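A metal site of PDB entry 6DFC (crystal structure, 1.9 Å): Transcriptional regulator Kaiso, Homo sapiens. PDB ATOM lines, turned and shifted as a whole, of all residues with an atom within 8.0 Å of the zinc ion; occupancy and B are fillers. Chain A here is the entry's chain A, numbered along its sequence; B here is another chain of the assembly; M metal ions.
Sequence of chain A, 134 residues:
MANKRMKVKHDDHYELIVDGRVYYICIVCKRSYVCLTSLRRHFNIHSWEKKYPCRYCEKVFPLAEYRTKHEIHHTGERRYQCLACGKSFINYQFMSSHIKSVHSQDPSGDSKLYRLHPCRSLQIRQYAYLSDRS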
ATOM      1  N   ASP A  12      10.077  20.356  -8.435  1.00  0.00           N
ATOM      2  CA  ASP A  12       9.201  20.443  -7.284  1.00  0.00           C
ATOM      3  C   ASP A  12       8.636  21.860  -7.192  1.00  0.00           C
ATOM      4  O   ASP A  12       7.900  22.191  -6.257  1.00  0.00           O
ATOM      5  CB  ASP A  12       9.951  20.071  -5.987  1.00  0.00           C
ATOM      6  CG  ASP A  12      11.265  20.849  -5.807  1.00  0.00           C
ATOM      7  OD1 ASP A  12      11.831  21.341  -6.804  1.00  0.00           O
ATOM      8  OD2 ASP A  12      11.752  20.929  -4.657  1.00  0.00           O
ATOM      9  N   ILE A  25       7.433  28.702  -6.332  1.00  0.00           N
ATOM     10  CA  ILE A  25       6.082  28.205  -6.105  1.00  0.00           C
ATOM     11  C   ILE A  25       6.042  26.689  -6.009  1.00  0.00           C
ATOM     12  O   ILE A  25       6.459  25.980  -6.929  1.00  0.00           O
ATOM     13  CB  ILE A  25       5.119  28.634  -7.246  1.00  0.00           C
ATOM     14  CG1 ILE A  25       5.331  30.106  -7.624  1.00  0.00           C
ATOM     15  CG2 ILE A  25       3.667  28.355  -6.844  1.00  0.00           C
ATOM     16  CD1 ILE A  25       5.055  31.072  -6.490  1.00  0.00           C
ATOM     17  N   CYS A  26       5.499  26.191  -4.915  1.00  0.00           N
ATOM     18  CA  CYS A  26       5.287  24.758  -4.784  1.00  0.00           C
ATOM     19  C   CYS A  26       4.311  24.242  -5.848  1.00  0.00           C
ATOM     20  O   CYS A  26       3.187  24.744  -5.952  1.00  0.00           O
ATOM     21  CB  CYS A  26       4.749  24.426  -3.411  1.00  0.00           C
ATOM     22  SG  CYS A  26       4.424  22.710  -3.254  1.00  0.00           S
ATOM     23  N   ILE A  27       4.707  23.238  -6.618  1.00  0.00           N
ATOM     24  CA  ILE A  27       3.842  22.730  -7.687  1.00  0.00           C
ATOM     25  C   ILE A  27       2.595  22.071  -7.118  1.00  0.00           C
ATOM     26  O   ILE A  27       1.570  22.016  -7.782  1.00  0.00           O
ATOM     27  CB  ILE A  27       4.564  21.708  -8.589  1.00  0.00           C
ATOM     28  CG1 ILE A  27       5.311  20.673  -7.743  1.00  0.00           C
ATOM     29  CG2 ILE A  27       5.509  22.415  -9.544  1.00  0.00           C
ATOM     30  CD1 ILE A  27       5.768  19.465  -8.527  1.00  0.00           C
ATOM     31  N   VAL A  28       2.663  21.605  -5.872  1.00  0.00           N
ATOM     32  CA  VAL A  28       1.545  20.836  -5.316  1.00  0.00           C
ATOM     33  C   VAL A  28       0.470  21.716  -4.700  1.00  0.00           C
ATOM     34  O   VAL A  28      -0.704  21.599  -5.062  1.00  0.00           O
ATOM     35  CB  VAL A  28       2.055  19.814  -4.266  1.00  0.00           C
ATOM     36  CG1 VAL A  28       0.884  19.220  -3.491  1.00  0.00           C
ATOM     37  CG2 VAL A  28       2.864  18.706  -4.937  1.00  0.00           C
ATOM     38  N   CYS A  29       0.857  22.619  -3.800  1.00  0.00           N
ATOM     39  CA  CYS A  29      -0.106  23.458  -3.083  1.00  0.00           C
ATOM     40  C   CYS A  29      -0.054  24.933  -3.478  1.00  0.00           C
ATOM     41  O   CYS A  29      -0.857  25.736  -3.000  1.00  0.00           O
ATOM     42  CB  CYS A  29       0.095  23.321  -1.564  1.00  0.00           C
ATOM     43  SG  CYS A  29       1.656  23.981  -0.931  1.00  0.00           S
ATOM     44  N   LYS A  30       0.912  25.290  -4.320  1.00  0.00           N
ATOM     45  CA  LYS A  30       1.086  26.643  -4.859  1.00  0.00           C
ATOM     46  C   LYS A  30       1.533  27.719  -3.847  1.00  0.00           C
ATOM     47  O   LYS A  30       1.402  28.912  -4.107  1.00  0.00           O
ATOM     48  CB  LYS A  30      -0.214  27.121  -5.528  1.00  0.00           C
ATOM     49  CG  LYS A  30      -0.715  26.247  -6.681  1.00  0.00           C
ATOM     50  CD  LYS A  30       0.205  26.310  -7.890  1.00  0.00           C
ATOM     51  CE  LYS A  30      -0.384  25.563  -9.111  1.00  0.00           C
ATOM     52  NZ  LYS A  30      -0.435  24.086  -8.941  1.00  0.00           N
ATOM     53  N   ARG A  31       2.087  27.314  -2.701  1.00  0.00           N
ATOM     54  CA  ARG A  31       2.618  28.292  -1.754  1.00  0.00           C
ATOM     55  C   ARG A  31       3.873  28.952  -2.335  1.00  0.00           C
ATOM     56  O   ARG A  31       4.643  28.294  -3.038  1.00  0.00           O
ATOM     57  CB  ARG A  31       2.936  27.656  -0.402  1.00  0.00           C
ATOM     58  CG  ARG A  31       1.708  27.367   0.434  1.00  0.00           C
ATOM     59  CD  ARG A  31       2.062  26.544   1.674  1.00  0.00           C
ATOM     60  NE  ARG A  31       0.874  26.057   2.355  1.00  0.00           N
ATOM     61  CZ  ARG A  31       0.316  26.652   3.394  1.00  0.00           C
ATOM     62  NH1 ARG A  31       0.847  27.768   3.894  1.00  0.00           N
ATOM     63  NH2 ARG A  31      -0.772  26.141   3.952  1.00  0.00           N
ATOM     64  N   SER A  32       4.073  30.235  -2.036  1.00  0.00           N
ATOM     65  CA  SER A  32       5.225  30.960  -2.567  1.00  0.00           C
ATOM     66  C   SER A  32       6.328  31.162  -1.536  1.00  0.00           C
ATOM     67  O   SER A  32       6.074  31.322  -0.340  1.00  0.00           O
ATOM     68  CB  SER A  32       4.786  32.322  -3.146  1.00  0.00           C
ATOM     69  OG  SER A  32       4.200  33.134  -2.162  1.00  0.00           O
ATOM     70  N   TYR A  33       7.565  31.121  -2.021  1.00  0.00           N
ATOM     71  CA  TYR A  33       8.731  31.210  -1.163  1.00  0.00           C
ATOM     72  C   TYR A  33       9.780  32.110  -1.792  1.00  0.00           C
ATOM     73  O   TYR A  33       9.995  32.095  -3.007  1.00  0.00           O
ATOM     74  CB  TYR A  33       9.293  29.816  -0.886  1.00  0.00           C
ATOM     75  CG  TYR A  33       8.297  28.915  -0.208  1.00  0.00           C
ATOM     76  CD1 TYR A  33       7.408  28.133  -0.942  1.00  0.00           C
ATOM     77  CD2 TYR A  33       8.211  28.892   1.185  1.00  0.00           C
ATOM     78  CE1 TYR A  33       6.478  27.334  -0.313  1.00  0.00           C
ATOM     79  CE2 TYR A  33       7.283  28.094   1.824  1.00  0.00           C
ATOM     80  CZ  TYR A  33       6.432  27.317   1.081  1.00  0.00           C
ATOM     81  OH  TYR A  33       5.501  26.549   1.729  1.00  0.00           O
ATOM     82  N   LEU A  39      11.345  26.323   0.131  1.00  0.00           N
ATOM     83  CA  LEU A  39      10.472  25.502  -0.697  1.00  0.00           C
ATOM     84  C   LEU A  39      10.783  24.045  -0.475  1.00  0.00           C
ATOM     85  O   LEU A  39       9.873  23.216  -0.330  1.00  0.00           O
ATOM     86  CB  LEU A  39      10.635  25.872  -2.183  1.00  0.00           C
ATOM     87  CG  LEU A  39       9.856  25.125  -3.281  1.00  0.00           C
ATOM     88  CD1 LEU A  39      10.576  23.853  -3.730  1.00  0.00           C
ATOM     89  CD2 LEU A  39       8.415  24.838  -2.881  1.00  0.00           C
ATOM     90  N   HIS A  42       9.810  22.897   2.966  1.00  0.00           N
ATOM     91  CA  HIS A  42       8.366  22.727   2.932  1.00  0.00           C
ATOM     92  C   HIS A  42       7.933  21.493   2.139  1.00  0.00           C
ATOM     93  O   HIS A  42       6.977  20.810   2.512  1.00  0.00           O
ATOM     94  CB  HIS A  42       7.713  23.962   2.323  1.00  0.00           C
ATOM     95  CG  HIS A  42       6.361  23.702   1.760  1.00  0.00           C
ATOM     96  ND1 HIS A  42       5.212  23.719   2.523  1.00  0.00           N
ATOM     97  CD2 HIS A  42       5.969  23.403   0.496  1.00  0.00           C
ATOM     98  CE1 HIS A  42       4.172  23.439   1.759  1.00  0.00           C
ATOM     99  NE2 HIS A  42       4.599  23.246   0.527  1.00  0.00           N
ATOM    100  N   PHE A  43       8.609  21.222   1.029  1.00  0.00           N
ATOM    101  CA  PHE A  43       8.100  20.207   0.110  1.00  0.00           C
ATOM    102  C   PHE A  43       8.096  18.812   0.726  1.00  0.00           C
ATOM    103  O   PHE A  43       7.353  17.935   0.293  1.00  0.00           O
ATOM    104  CB  PHE A  43       8.917  20.201  -1.196  1.00  0.00           C
ATOM    105  CG  PHE A  43       8.230  19.479  -2.325  1.00  0.00           C
ATOM    106  CD1 PHE A  43       7.218  20.096  -3.042  1.00  0.00           C
ATOM    107  CD2 PHE A  43       8.607  18.201  -2.689  1.00  0.00           C
ATOM    108  CE1 PHE A  43       6.589  19.455  -4.085  1.00  0.00           C
ATOM    109  CE2 PHE A  43       7.989  17.542  -3.743  1.00  0.00           C
ATOM    110  CZ  PHE A  43       6.968  18.167  -4.449  1.00  0.00           C
ATOM    111  N   ASN A  44       8.895  18.609   1.769  1.00  0.00           N
ATOM    112  CA  ASN A  44       8.953  17.306   2.409  1.00  0.00           C
ATOM    113  C   ASN A  44       7.587  16.890   2.952  1.00  0.00           C
ATOM    114  O   ASN A  44       7.294  15.707   3.090  1.00  0.00           O
ATOM    115  CB  ASN A  44       9.990  17.274   3.526  1.00  0.00           C
ATOM    116  CG  ASN A  44      10.373  15.851   3.905  1.00  0.00           C
ATOM    117  OD1 ASN A  44      10.826  15.078   3.051  1.00  0.00           O
ATOM    118  ND2 ASN A  44      10.177  15.504   5.172  1.00  0.00           N
ATOM    119  N   ILE A  45       6.770  17.892   3.282  1.00  0.00           N
ATOM    120  CA  ILE A  45       5.405  17.658   3.734  1.00  0.00           C
ATOM    121  C   ILE A  45       4.607  16.898   2.683  1.00  0.00           C
ATOM    122  O   ILE A  45       3.784  16.044   3.014  1.00  0.00           O
ATOM    123  CB  ILE A  45       4.709  18.984   4.053  1.00  0.00           C
ATOM    124  CG1 ILE A  45       5.442  19.693   5.193  1.00  0.00           C
ATOM    125  CG2 ILE A  45       3.244  18.763   4.394  1.00  0.00           C
ATOM    126  CD1 ILE A  45       5.049  21.129   5.328  1.00  0.00           C
ATOM    127  N   HIS A  46       4.862  17.215   1.424  1.00  0.00           N
ATOM    128  CA  HIS A  46       4.229  16.502   0.314  1.00  0.00           C
ATOM    129  C   HIS A  46       4.904  15.152   0.021  1.00  0.00           C
ATOM    130  O   HIS A  46       4.234  14.128  -0.063  1.00  0.00           O
ATOM    131  CB  HIS A  46       4.257  17.369  -0.950  1.00  0.00           C
ATOM    132  CG  HIS A  46       3.600  18.700  -0.773  1.00  0.00           C
ATOM    133  ND1 HIS A  46       2.409  18.852  -0.099  1.00  0.00           N
ATOM    134  CD2 HIS A  46       3.970  19.935  -1.176  1.00  0.00           C
ATOM    135  CE1 HIS A  46       2.060  20.132  -0.110  1.00  0.00           C
ATOM    136  NE2 HIS A  46       2.997  20.810  -0.756  1.00  0.00           N
ATOM    137  P    DT B   8       4.828  28.649   4.550  1.00  0.00           P
ATOM    138  OP1  DT B   8       3.901  29.339   3.616  1.00  0.00           O
ATOM    139  OP2  DT B   8       5.220  27.242   4.250  1.00  0.00           O
ATOM    140  O5'  DT B   8       6.124  29.536   4.729  1.00  0.00           O
ATOM    141  C5'  DT B   8       5.982  30.923   4.924  1.00  0.00           C
ATOM    142  C4'  DT B   8       7.305  31.531   5.293  1.00  0.00           C
ATOM    143  O4'  DT B   8       7.667  31.157   6.665  1.00  0.00           O
ATOM    144  C3'  DT B   8       8.492  31.124   4.416  1.00  0.00           C
ATOM    145  O3'  DT B   8       9.316  32.253   4.246  1.00  0.00           O
ATOM    146  C2'  DT B   8       9.181  30.060   5.306  1.00  0.00           C
ATOM    147  C1'  DT B   8       9.001  30.740   6.658  1.00  0.00           C
ATOM    148  N1   DT B   8       9.211  29.883   7.880  1.00  0.00           N
ATOM    149  C2   DT B   8       9.521  30.511   9.064  1.00  0.00           C
ATOM    150  O2   DT B   8       9.675  31.714   9.151  1.00  0.00           O
ATOM    151  N3   DT B   8       9.670  29.693  10.134  1.00  0.00           N
ATOM    152  C4   DT B   8       9.519  28.330  10.176  1.00  0.00           C
ATOM    153  O4   DT B   8       9.684  27.687  11.214  1.00  0.00           O
ATOM    154  C5   DT B   8       9.189  27.718   8.913  1.00  0.00           C
ATOM    155  C7   DT B   8       9.012  26.238   8.844  1.00  0.00           C
ATOM    156  C6   DT B   8       9.028  28.513   7.817  1.00  0.00           C
HETATM  157 ZN    ZN M   1       3.440  22.695  -1.142  1.00  0.00          ZN
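The backbone NH of Cys 26 is in hydrogen-bond range of the backbone carbonyl oxygen of Arg 31, at 2.9 Å.
The backbone NH (N) of Arg 31 sits close to the side-chain sulfur (SG) of Cys 29 (3.8 Å).
The side-chain sulfur (SG) of Cys 26 sits close to the backbone NH (N) of Val 28, at 3.3 Å.
A ring nitrogen (ND1) of His 42 lies within hydrogen-bond range of the side-chain hydroxyl (OH) of Tyr 33 (3.0 Å).
Four residues have an atom within 4 Å of the zinc ion: Cys 26, Cys 29, His 42 and His 46.
Along chain A the residues within 4 Å of the zinc ion span positions 26 to 46.
The nearest printed residue that does not touch the zinc ion is Val 28 (4.5 Å).
The zinc ion is bound by a ring nitrogen (NE2) of His 46 (2.0 Å).
NE2 of His 42 binds the zinc ion (2.1 Å).
The zinc ion is bound by SG of Cys 29, at 2.2 Å.
The side-chain sulfur (SG) of Cys 26 is bound to the zinc ion (2.3 Å).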
